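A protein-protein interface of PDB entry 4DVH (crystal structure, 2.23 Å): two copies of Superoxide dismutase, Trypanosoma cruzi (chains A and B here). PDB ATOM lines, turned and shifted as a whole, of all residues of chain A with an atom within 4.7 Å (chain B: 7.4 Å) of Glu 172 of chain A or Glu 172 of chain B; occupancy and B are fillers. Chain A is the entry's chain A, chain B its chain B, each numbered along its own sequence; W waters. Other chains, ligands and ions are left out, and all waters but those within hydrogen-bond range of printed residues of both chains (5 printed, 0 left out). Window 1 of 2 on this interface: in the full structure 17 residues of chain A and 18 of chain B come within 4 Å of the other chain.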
ATOM      1  N   HIS A  38     -20.233  30.738  25.317  1.00  0.00           N
ATOM      2  CA  HIS A  38     -20.872  30.254  24.099  1.00  0.00           C
ATOM      3  C   HIS A  38     -21.729  31.326  23.411  1.00  0.00           C
ATOM      4  O   HIS A  38     -21.436  31.663  22.271  1.00  0.00           O
ATOM      5  CB  HIS A  38     -21.664  28.947  24.350  1.00  0.00           C
ATOM      6  CG  HIS A  38     -20.797  27.813  24.812  1.00  0.00           C
ATOM      7  ND1 HIS A  38     -20.064  27.062  23.919  1.00  0.00           N
ATOM      8  CD2 HIS A  38     -20.534  27.382  26.066  1.00  0.00           C
ATOM      9  CE1 HIS A  38     -19.392  26.188  24.647  1.00  0.00           C
ATOM     10  NE2 HIS A  38     -19.656  26.329  25.942  1.00  0.00           N
ATOM     11  N   VAL A 170     -29.833  21.236  22.858  1.00  0.00           N
ATOM     12  CA  VAL A 170     -29.319  19.881  23.104  1.00  0.00           C
ATOM     13  C   VAL A 170     -27.840  19.723  22.710  1.00  0.00           C
ATOM     14  O   VAL A 170     -27.317  18.606  22.677  1.00  0.00           O
ATOM     15  CB  VAL A 170     -30.251  18.683  22.729  1.00  0.00           C
ATOM     16  CG1 VAL A 170     -31.560  18.751  23.492  1.00  0.00           C
ATOM     17  CG2 VAL A 170     -30.503  18.586  21.222  1.00  0.00           C
ATOM     18  N   TRP A 171     -27.153  20.870  22.422  1.00  0.00           N
ATOM     19  CA  TRP A 171     -25.697  20.886  22.214  1.00  0.00           C
ATOM     20  C   TRP A 171     -25.196  20.485  23.603  1.00  0.00           C
ATOM     21  O   TRP A 171     -25.813  20.882  24.603  1.00  0.00           O
ATOM     22  CB  TRP A 171     -25.200  22.303  21.908  1.00  0.00           C
ATOM     23  CG  TRP A 171     -25.277  22.723  20.466  1.00  0.00           C
ATOM     24  CD1 TRP A 171     -26.409  22.940  19.730  1.00  0.00           C
ATOM     25  CD2 TRP A 171     -24.173  23.139  19.641  1.00  0.00           C
ATOM     26  NE1 TRP A 171     -26.078  23.416  18.479  1.00  0.00           N
ATOM     27  CE2 TRP A 171     -24.711  23.563  18.404  1.00  0.00           C
ATOM     28  CE3 TRP A 171     -22.775  23.180  19.825  1.00  0.00           C
ATOM     29  CZ2 TRP A 171     -23.894  24.002  17.341  1.00  0.00           C
ATOM     30  CZ3 TRP A 171     -21.973  23.624  18.776  1.00  0.00           C
ATOM     31  CH2 TRP A 171     -22.531  24.031  17.554  1.00  0.00           C
ATOM     32  N   GLU A 172     -24.155  19.660  23.682  1.00  0.00           N
ATOM     33  CA  GLU A 172     -23.668  19.129  24.971  1.00  0.00           C
ATOM     34  C   GLU A 172     -23.286  20.183  25.991  1.00  0.00           C
ATOM     35  O   GLU A 172     -23.499  19.973  27.187  1.00  0.00           O
ATOM     36  CB  GLU A 172     -22.555  18.096  24.767  1.00  0.00           C
ATOM     37  CG  GLU A 172     -22.970  16.914  23.888  1.00  0.00           C
ATOM     38  CD  GLU A 172     -21.864  15.903  23.694  1.00  0.00           C
ATOM     39  OE1 GLU A 172     -20.742  16.312  23.320  1.00  0.00           O
ATOM     40  OE2 GLU A 172     -22.099  14.714  23.994  1.00  0.00           O
ATOM     41  N   HIS A 173     -22.745  21.323  25.530  1.00  0.00           N
ATOM     42  CA  HIS A 173     -22.379  22.466  26.391  1.00  0.00           C
ATOM     43  C   HIS A 173     -23.560  23.024  27.190  1.00  0.00           C
ATOM     44  O   HIS A 173     -23.323  23.686  28.206  1.00  0.00           O
ATOM     45  CB  HIS A 173     -21.705  23.613  25.585  1.00  0.00           C
ATOM     46  CG  HIS A 173     -22.578  24.338  24.592  1.00  0.00           C
ATOM     47  ND1 HIS A 173     -22.193  24.480  23.262  1.00  0.00           N
ATOM     48  CD2 HIS A 173     -23.731  25.025  24.778  1.00  0.00           C
ATOM     49  CE1 HIS A 173     -23.136  25.210  22.684  1.00  0.00           C
ATOM     50  NE2 HIS A 173     -24.085  25.554  23.550  1.00  0.00           N
ATOM     51  N   ALA A 174     -24.831  22.787  26.721  1.00  0.00           N
ATOM     52  CA  ALA A 174     -26.023  23.294  27.407  1.00  0.00           C
ATOM     53  C   ALA A 174     -26.258  22.623  28.754  1.00  0.00           C
ATOM     54  O   ALA A 174     -26.893  23.217  29.631  1.00  0.00           O
ATOM     55  CB  ALA A 174     -27.254  23.122  26.535  1.00  0.00           C
ATOM     56  N   TYR A 175     -25.781  21.373  28.915  1.00  0.00           N
ATOM     57  CA  TYR A 175     -26.020  20.598  30.118  1.00  0.00           C
ATOM     58  C   TYR A 175     -24.805  19.906  30.737  1.00  0.00           C
ATOM     59  O   TYR A 175     -24.945  19.351  31.827  1.00  0.00           O
ATOM     60  CB  TYR A 175     -27.118  19.553  29.837  1.00  0.00           C
ATOM     61  CG  TYR A 175     -26.807  18.588  28.702  1.00  0.00           C
ATOM     62  CD1 TYR A 175     -26.085  17.420  28.932  1.00  0.00           C
ATOM     63  CD2 TYR A 175     -27.282  18.816  27.417  1.00  0.00           C
ATOM     64  CE1 TYR A 175     -25.801  16.532  27.892  1.00  0.00           C
ATOM     65  CE2 TYR A 175     -27.007  17.938  26.378  1.00  0.00           C
ATOM     66  CZ  TYR A 175     -26.266  16.798  26.617  1.00  0.00           C
ATOM     67  OH  TYR A 175     -26.022  15.930  25.587  1.00  0.00           O
ATOM     68  N   TYR A 176     -23.649  19.871  30.041  1.00  0.00           N
ATOM     69  CA  TYR A 176     -22.485  19.095  30.504  1.00  0.00           C
ATOM     70  C   TYR A 176     -21.928  19.421  31.879  1.00  0.00           C
ATOM     71  O   TYR A 176     -21.399  18.536  32.557  1.00  0.00           O
ATOM     72  CB  TYR A 176     -21.381  18.965  29.444  1.00  0.00           C
ATOM     73  CG  TYR A 176     -20.824  17.554  29.355  1.00  0.00           C
ATOM     74  CD1 TYR A 176     -21.406  16.608  28.523  1.00  0.00           C
ATOM     75  CD2 TYR A 176     -19.730  17.159  30.129  1.00  0.00           C
ATOM     76  CE1 TYR A 176     -20.930  15.306  28.464  1.00  0.00           C
ATOM     77  CE2 TYR A 176     -19.220  15.863  30.051  1.00  0.00           C
ATOM     78  CZ  TYR A 176     -19.845  14.931  29.240  1.00  0.00           C
ATOM     79  OH  TYR A 176     -19.395  13.639  29.169  1.00  0.00           O
ATOM     80  N   GLN B  30     -13.009  12.885  33.271  1.00  0.00           N
ATOM     81  CA  GLN B  30     -13.133  13.100  31.819  1.00  0.00           C
ATOM     82  C   GLN B  30     -13.010  11.758  31.070  1.00  0.00           C
ATOM     83  O   GLN B  30     -13.773  11.506  30.145  1.00  0.00           O
ATOM     84  CB  GLN B  30     -12.053  14.077  31.310  1.00  0.00           C
ATOM     85  CG  GLN B  30     -12.106  14.372  29.805  1.00  0.00           C
ATOM     86  CD  GLN B  30     -13.335  15.148  29.408  1.00  0.00           C
ATOM     87  OE1 GLN B  30     -13.370  16.375  29.486  1.00  0.00           O
ATOM     88  NE2 GLN B  30     -14.384  14.452  28.984  1.00  0.00           N
ATOM     89  N   HIS B  38     -20.175   7.550  27.375  1.00  0.00           N
ATOM     90  CA  HIS B  38     -20.331   7.805  25.936  1.00  0.00           C
ATOM     91  C   HIS B  38     -19.969   6.619  25.075  1.00  0.00           C
ATOM     92  O   HIS B  38     -20.830   6.137  24.340  1.00  0.00           O
ATOM     93  CB  HIS B  38     -19.569   9.082  25.487  1.00  0.00           C
ATOM     94  CG  HIS B  38     -20.084  10.322  26.155  1.00  0.00           C
ATOM     95  ND1 HIS B  38     -21.215  10.961  25.703  1.00  0.00           N
ATOM     96  CD2 HIS B  38     -19.629  10.961  27.260  1.00  0.00           C
ATOM     97  CE1 HIS B  38     -21.401  11.984  26.518  1.00  0.00           C
ATOM     98  NE2 HIS B  38     -20.458  12.034  27.464  1.00  0.00           N
ATOM     99  N   TYR B  42     -22.528   3.815  22.949  1.00  0.00           N
ATOM    100  CA  TYR B  42     -22.421   3.555  21.502  1.00  0.00           C
ATOM    101  C   TYR B  42     -22.341   2.054  21.275  1.00  0.00           C
ATOM    102  O   TYR B  42     -23.018   1.529  20.387  1.00  0.00           O
ATOM    103  CB  TYR B  42     -21.184   4.263  20.881  1.00  0.00           C
ATOM    104  CG  TYR B  42     -21.335   5.764  20.754  1.00  0.00           C
ATOM    105  CD1 TYR B  42     -22.424   6.324  20.075  1.00  0.00           C
ATOM    106  CD2 TYR B  42     -20.411   6.626  21.331  1.00  0.00           C
ATOM    107  CE1 TYR B  42     -22.573   7.710  19.969  1.00  0.00           C
ATOM    108  CE2 TYR B  42     -20.562   8.009  21.252  1.00  0.00           C
ATOM    109  CZ  TYR B  42     -21.628   8.547  20.546  1.00  0.00           C
ATOM    110  OH  TYR B  42     -21.745   9.913  20.432  1.00  0.00           O
ATOM    111  N   GLY B 130     -19.915  22.344  15.408  1.00  0.00           N
ATOM    112  CA  GLY B 130     -20.727  21.391  16.140  1.00  0.00           C
ATOM    113  C   GLY B 130     -19.928  20.184  16.590  1.00  0.00           C
ATOM    114  O   GLY B 130     -18.734  20.299  16.917  1.00  0.00           O
ATOM    115  N   SER B 131     -20.585  19.012  16.595  1.00  0.00           N
ATOM    116  CA  SER B 131     -19.974  17.755  16.995  1.00  0.00           C
ATOM    117  C   SER B 131     -19.240  17.184  15.793  1.00  0.00           C
ATOM    118  O   SER B 131     -19.776  17.212  14.672  1.00  0.00           O
ATOM    119  CB  SER B 131     -21.055  16.791  17.460  1.00  0.00           C
ATOM    120  OG  SER B 131     -21.692  17.295  18.623  1.00  0.00           O
ATOM    121  N   GLY B 132     -18.031  16.675  16.025  1.00  0.00           N
ATOM    122  CA  GLY B 132     -17.232  16.086  14.962  1.00  0.00           C
ATOM    123  C   GLY B 132     -15.908  15.467  15.354  1.00  0.00           C
ATOM    124  O   GLY B 132     -15.622  15.205  16.528  1.00  0.00           O
ATOM    125  N   ASP B 169     -11.273  13.622  18.732  1.00  0.00           N
ATOM    126  CA  ASP B 169     -12.690  13.877  18.979  1.00  0.00           C
ATOM    127  C   ASP B 169     -12.903  15.353  19.312  1.00  0.00           C
ATOM    128  O   ASP B 169     -12.231  15.887  20.200  1.00  0.00           O
ATOM    129  CB  ASP B 169     -13.169  13.000  20.150  1.00  0.00           C
ATOM    130  CG  ASP B 169     -14.672  12.823  20.291  1.00  0.00           C
ATOM    131  OD1 ASP B 169     -15.433  13.520  19.573  1.00  0.00           O
ATOM    132  OD2 ASP B 169     -15.083  11.970  21.082  1.00  0.00           O
ATOM    133  N   VAL B 170     -13.821  16.008  18.588  1.00  0.00           N
ATOM    134  CA  VAL B 170     -14.188  17.404  18.848  1.00  0.00           C
ATOM    135  C   VAL B 170     -15.649  17.575  19.301  1.00  0.00           C
ATOM    136  O   VAL B 170     -16.153  18.693  19.365  1.00  0.00           O
ATOM    137  CB  VAL B 170     -13.663  18.478  17.858  1.00  0.00           C
ATOM    138  CG1 VAL B 170     -12.152  18.467  17.795  1.00  0.00           C
ATOM    139  CG2 VAL B 170     -14.263  18.324  16.468  1.00  0.00           C
ATOM    140  N   TRP B 171     -16.328  16.446  19.623  1.00  0.00           N
ATOM    141  CA  TRP B 171     -17.662  16.471  20.225  1.00  0.00           C
ATOM    142  C   TRP B 171     -17.341  17.113  21.574  1.00  0.00           C
ATOM    143  O   TRP B 171     -16.271  16.849  22.126  1.00  0.00           O
ATOM    144  CB  TRP B 171     -18.189  15.044  20.460  1.00  0.00           C
ATOM    145  CG  TRP B 171     -18.891  14.408  19.285  1.00  0.00           C
ATOM    146  CD1 TRP B 171     -18.323  14.004  18.107  1.00  0.00           C
ATOM    147  CD2 TRP B 171     -20.240  13.927  19.265  1.00  0.00           C
ATOM    148  NE1 TRP B 171     -19.262  13.360  17.322  1.00  0.00           N
ATOM    149  CE2 TRP B 171     -20.446  13.295  18.013  1.00  0.00           C
ATOM    150  CE3 TRP B 171     -21.312  14.009  20.167  1.00  0.00           C
ATOM    151  CZ2 TRP B 171     -21.689  12.748  17.641  1.00  0.00           C
ATOM    152  CZ3 TRP B 171     -22.538  13.453  19.804  1.00  0.00           C
ATOM    153  CH2 TRP B 171     -22.718  12.843  18.555  1.00  0.00           C
ATOM    154  N   GLU B 172     -18.215  18.003  22.068  1.00  0.00           N
ATOM    155  CA  GLU B 172     -17.961  18.752  23.308  1.00  0.00           C
ATOM    156  C   GLU B 172     -17.688  17.878  24.526  1.00  0.00           C
ATOM    157  O   GLU B 172     -16.892  18.260  25.383  1.00  0.00           O
ATOM    158  CB  GLU B 172     -19.082  19.790  23.567  1.00  0.00           C
ATOM    159  CG  GLU B 172     -19.259  20.783  22.434  1.00  0.00           C
ATOM    160  CD  GLU B 172     -20.323  21.831  22.692  1.00  0.00           C
ATOM    161  OE1 GLU B 172     -21.471  21.462  23.017  1.00  0.00           O
ATOM    162  OE2 GLU B 172     -20.011  23.035  22.572  1.00  0.00           O
ATOM    163  N   HIS B 173     -18.327  16.703  24.597  1.00  0.00           N
ATOM    164  CA  HIS B 173     -18.126  15.736  25.699  1.00  0.00           C
ATOM    165  C   HIS B 173     -16.678  15.243  25.814  1.00  0.00           C
ATOM    166  O   HIS B 173     -16.306  14.740  26.872  1.00  0.00           O
ATOM    167  CB  HIS B 173     -19.083  14.525  25.584  1.00  0.00           C
ATOM    168  CG  HIS B 173     -18.861  13.603  24.409  1.00  0.00           C
ATOM    169  ND1 HIS B 173     -19.900  13.281  23.545  1.00  0.00           N
ATOM    170  CD2 HIS B 173     -17.769  12.888  24.052  1.00  0.00           C
ATOM    171  CE1 HIS B 173     -19.396  12.406  22.680  1.00  0.00           C
ATOM    172  NE2 HIS B 173     -18.115  12.155  22.930  1.00  0.00           N
ATOM    173  N   ALA B 174     -15.873  15.348  24.717  1.00  0.00           N
ATOM    174  CA  ALA B 174     -14.487  14.882  24.729  1.00  0.00           C
ATOM    175  C   ALA B 174     -13.598  15.740  25.612  1.00  0.00           C
ATOM    176  O   ALA B 174     -12.582  15.262  26.092  1.00  0.00           O
ATOM    177  CB  ALA B 174     -13.935  14.853  23.320  1.00  0.00           C
ATOM    178  N   TYR B 175     -13.972  17.008  25.822  1.00  0.00           N
ATOM    179  CA  TYR B 175     -13.147  17.962  26.574  1.00  0.00           C
ATOM    180  C   TYR B 175     -13.875  18.804  27.626  1.00  0.00           C
ATOM    181  O   TYR B 175     -13.191  19.504  28.367  1.00  0.00           O
ATOM    182  CB  TYR B 175     -12.420  18.903  25.587  1.00  0.00           C
ATOM    183  CG  TYR B 175     -13.336  19.688  24.664  1.00  0.00           C
ATOM    184  CD1 TYR B 175     -13.884  20.911  25.062  1.00  0.00           C
ATOM    185  CD2 TYR B 175     -13.621  19.233  23.378  1.00  0.00           C
ATOM    186  CE1 TYR B 175     -14.718  21.637  24.220  1.00  0.00           C
ATOM    187  CE2 TYR B 175     -14.458  19.951  22.526  1.00  0.00           C
ATOM    188  CZ  TYR B 175     -14.999  21.156  22.949  1.00  0.00           C
ATOM    189  OH  TYR B 175     -15.786  21.882  22.102  1.00  0.00           O
ATOM    190  N   TYR B 176     -15.228  18.792  27.663  1.00  0.00           N
ATOM    191  CA  TYR B 176     -15.994  19.673  28.550  1.00  0.00           C
ATOM    192  C   TYR B 176     -15.722  19.590  30.029  1.00  0.00           C
ATOM    193  O   TYR B 176     -15.847  20.593  30.722  1.00  0.00           O
ATOM    194  CB  TYR B 176     -17.505  19.693  28.236  1.00  0.00           C
ATOM    195  CG  TYR B 176     -18.073  21.100  28.231  1.00  0.00           C
ATOM    196  CD1 TYR B 176     -18.078  21.871  27.067  1.00  0.00           C
ATOM    197  CD2 TYR B 176     -18.615  21.660  29.388  1.00  0.00           C
ATOM    198  CE1 TYR B 176     -18.571  23.173  27.063  1.00  0.00           C
ATOM    199  CE2 TYR B 176     -19.141  22.950  29.387  1.00  0.00           C
ATOM    200  CZ  TYR B 176     -19.092  23.711  28.227  1.00  0.00           C
ATOM    201  OH  TYR B 176     -19.564  24.998  28.211  1.00  0.00           O
ATOM    202  N   LYS B 177     -15.327  18.420  30.516  1.00  0.00           N
ATOM    203  CA  LYS B 177     -15.038  18.243  31.930  1.00  0.00           C
ATOM    204  C   LYS B 177     -13.711  18.930  32.302  1.00  0.00           C
ATOM    205  O   LYS B 177     -13.662  19.654  33.296  1.00  0.00           O
ATOM    206  CB  LYS B 177     -15.059  16.734  32.318  1.00  0.00           C
ATOM    207  CG  LYS B 177     -14.697  16.413  33.783  1.00  0.00           C
ATOM    208  CD  LYS B 177     -15.623  17.037  34.840  1.00  0.00           C
ATOM    209  CE  LYS B 177     -16.979  16.373  34.904  1.00  0.00           C
ATOM    210  NZ  LYS B 177     -17.769  16.826  36.077  1.00  0.00           N
ATOM    211  N   GLU B 180     -13.958  22.798  29.586  1.00  0.00           N
ATOM    212  CA  GLU B 180     -15.223  23.520  29.401  1.00  0.00           C
ATOM    213  C   GLU B 180     -15.346  23.978  27.922  1.00  0.00           C
ATOM    214  O   GLU B 180     -15.063  23.183  27.045  1.00  0.00           O
ATOM    215  CB  GLU B 180     -15.361  24.660  30.440  1.00  0.00           C
ATOM    216  CG  GLU B 180     -15.354  24.155  31.876  1.00  0.00           C
ATOM    217  CD  GLU B 180     -15.191  25.248  32.911  1.00  0.00           C
ATOM    218  OE1 GLU B 180     -14.295  26.102  32.733  1.00  0.00           O
ATOM    219  OE2 GLU B 180     -15.947  25.248  33.909  1.00  0.00           O
ATOM    220  N   ASN B 181     -15.693  25.243  27.647  1.00  0.00           N
ATOM    221  CA  ASN B 181     -15.832  25.807  26.296  1.00  0.00           C
ATOM    222  C   ASN B 181     -14.499  25.934  25.511  1.00  0.00           C
ATOM    223  O   ASN B 181     -14.536  26.315  24.326  1.00  0.00           O
ATOM    224  CB  ASN B 181     -16.408  27.228  26.429  1.00  0.00           C
ATOM    225  CG  ASN B 181     -15.446  28.162  27.102  1.00  0.00           C
ATOM    226  OD1 ASN B 181     -15.167  28.035  28.295  1.00  0.00           O
ATOM    227  ND2 ASN B 181     -14.870  29.071  26.331  1.00  0.00           N
ATOM    228  N   ARG B 183     -12.222  24.592  23.529  1.00  0.00           N
ATOM    229  CA  ARG B 183     -11.803  23.658  22.488  1.00  0.00           C
ATOM    230  C   ARG B 183     -10.388  23.979  21.960  1.00  0.00           C
ATOM    231  O   ARG B 183      -9.615  23.029  21.833  1.00  0.00           O
ATOM    232  CB  ARG B 183     -12.810  23.582  21.326  1.00  0.00           C
ATOM    233  CG  ARG B 183     -12.503  22.378  20.431  1.00  0.00           C
ATOM    234  CD  ARG B 183     -13.212  22.474  19.114  1.00  0.00           C
ATOM    235  NE  ARG B 183     -14.600  22.078  19.277  1.00  0.00           N
ATOM    236  CZ  ARG B 183     -15.452  21.889  18.279  1.00  0.00           C
ATOM    237  NH1 ARG B 183     -15.066  22.056  17.031  1.00  0.00           N
ATOM    238  NH2 ARG B 183     -16.693  21.520  18.525  1.00  0.00           N
ATOM    239  N   TYR B 186      -7.817  22.524  24.462  1.00  0.00           N
ATOM    240  CA  TYR B 186      -7.862  21.056  24.379  1.00  0.00           C
ATOM    241  C   TYR B 186      -7.028  20.572  23.203  1.00  0.00           C
ATOM    242  O   TYR B 186      -6.221  19.650  23.349  1.00  0.00           O
ATOM    243  CB  TYR B 186      -9.329  20.594  24.258  1.00  0.00           C
ATOM    244  CG  TYR B 186      -9.554  19.226  23.632  1.00  0.00           C
ATOM    245  CD1 TYR B 186      -9.214  18.062  24.311  1.00  0.00           C
ATOM    246  CD2 TYR B 186     -10.192  19.098  22.396  1.00  0.00           C
ATOM    247  CE1 TYR B 186      -9.516  16.801  23.788  1.00  0.00           C
ATOM    248  CE2 TYR B 186     -10.463  17.844  21.842  1.00  0.00           C
ATOM    249  CZ  TYR B 186     -10.128  16.698  22.547  1.00  0.00           C
ATOM    250  OH  TYR B 186     -10.380  15.460  22.029  1.00  0.00           O
HETATM  251  O   HOH W   1     -20.888  17.730  21.052  1.00  0.00           O
HETATM  252  O   HOH W   2     -22.260  26.074  28.714  1.00  0.00           O
HETATM  253  O   HOH W   3     -22.676  19.557  21.295  1.00  0.00           O
HETATM  254  O   HOH W   4     -18.823  18.581  33.409  1.00  0.00           O
HETATM  255  O   HOH W   5     -16.867  12.669  28.188  1.00  0.00           O
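NE2 of His 38 of chain A lies within hydrogen-bond range of OH of Tyr 176 of chain B. OE1 of Glu 172 of chain A sits at hydrogen-bond distance from N of Glu 172 of chain B, at 3.3 Å. The side-chain carboxylate (OE2) of Glu 172 of chain A sits at hydrogen-bond distance from a ring nitrogen (ND1) of His 173 of chain B (2.7 Å). A ring nitrogen (ND1) of His 173 of chain A lies within hydrogen-bond range of the side-chain carboxylate (OE2) of Glu 172 of chain B (2.7 Å). OH of Tyr 176 of chain A sits at hydrogen-bond distance from NE2 of His 38 of chain B (2.6 Å).
ND1 of His 173 of chain A lies within hydrogen-bond range of ND1 of His 38 of chain A (3.4 Å). The side-chain amide nitrogen of Gln 30 of chain B is in hydrogen-bond range of the backbone carbonyl oxygen of His 173 of chain B, 2.9 Å away. ND1 of His 173 of chain B lies within hydrogen-bond range of ND1 of His 38 of chain B (3.4 Å). The guanidinium group of Arg 183 of chain B sits at hydrogen-bond distance from the backbone carbonyl oxygen of Gly 130 of chain B. The backbone carbonyl oxygen of Gly 132 of chain B lies close to the backbone NH of Trp 171 of chain B (3.4 Å). The side-chain carboxylate (OD1) of Asp 169 of chain B lies within hydrogen-bond range of the backbone NH (N) of Trp 171 of chain B, 3.1 Å away.
His 38 of chain A touches Glu 172 of chain B (CE1 to OE2, 3.8 Å). His 38 of chain A touches Asn 181 of chain B (NE2 to CB, 3.4 Å). Trp 171 of chain A touches Gly 130 of chain B (CH2 to CA, 3.5 Å). Trp 171 of chain A touches Glu 172 of chain B (CE3 to OE1, 3.9 Å). OE2 of Glu 172 of chain A touches CE1 of His 38 of chain B, 3.8 Å away. Glu 172 of chain A touches Trp 171 of chain B (OE1 to C, 3.9 Å). His 173 of chain A touches Tyr 176 of chain B (CB to CE1, 3.5 Å). CE1 of Tyr 176 of chain A touches CB of His 173 of chain B, 3.5 Å away. Tyr 176 of chain A touches Tyr 176 of chain B (CB to CD2, 3.9 Å).
Of the printed residues of chain B, Glu 172 of chain A touches His 38 (3.8 Å), Trp 171 (3.9 Å), Glu 172 (3.3 Å) and His 173 (2.7 Å). Of chain A, only His 38 (3.8 Å), Trp 171 (3.9 Å), Glu 172 (3.3 Å) and His 173 (2.7 Å) come within 4 Å of Glu 172 of chain B. Printed residues of chain A within 4 Å of His 38 of chain B: Glu 172 (3.8 Å) and Tyr 176 (2.6 Å). Of the printed residues of chain B, His 173 of chain A touches Glu 172 and Tyr 176. Printed residues of chain A within 4 Å of His 173 of chain B: Glu 172 (2.7 Å) and Tyr 176 (3.5 Å). Of the printed residues of chain A, Tyr 176 of chain B touches His 38 (2.6 Å), His 173 (3.5 Å) and Tyr 176 (3.9 Å). Glu 180 of chain B touches none of the printed residues of chain A. Gly 132 of chain B touches none of the printed residues of chain A. The nearest residue of chain B that does not touch Glu 172 of chain A is Ser 131 of chain B (4.9 Å).
Hydrophobic or aromatic side chains of chain A that line the printed part of chain B: His 38, Trp 171, His 173 and Tyr 176.
His 38 of chain A touches Glu 172 of chain B, and with the chains exchanged Glu 172 of chain A touches His 38 of chain B. Trp 171 of chain A touches Glu 172 of chain B, and with the chains exchanged Glu 172 of chain A touches Trp 171 of chain B. Glu 172 of chain B touches its own counterpart, Glu 172 of chain A. His 173 of chain A touches Tyr 176 of chain B, and with the chains exchanged Tyr 176 of chain A touches His 173 of chain B. 8 positions are printed for both chains. Of the 14 pairs that touch across the chains among the printed residues, 12 have their exchanged pair printed and touching as well.
Water W5 lies within hydrogen-bond range of O of His 173 of chain B (2.5 Å), OH of Tyr 176 of chain A (2.9 Å) and NE2 of Gln 30 of chain B (3.2 Å). Water W1 lies within hydrogen-bond range of OG of Ser 131 of chain B (2.6 Å), OE1 of Glu 172 of chain A (2.7 Å) and N of Glu 172 of chain B (2.9 Å). Water W2 bridges the backbone carbonyl oxygen (O) of His 173 of chain A (2.7 Å) and the side-chain hydroxyl (OH) of Tyr 176 of chain B (2.9 Å). Water W4 bridges O of Tyr 176 of chain A (2.7 Å) and NZ of Lys 177 of chain B (3.4 Å). Water W3 bridges N of Glu 172 of chain A and OE1 of Glu 172 of chain B.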
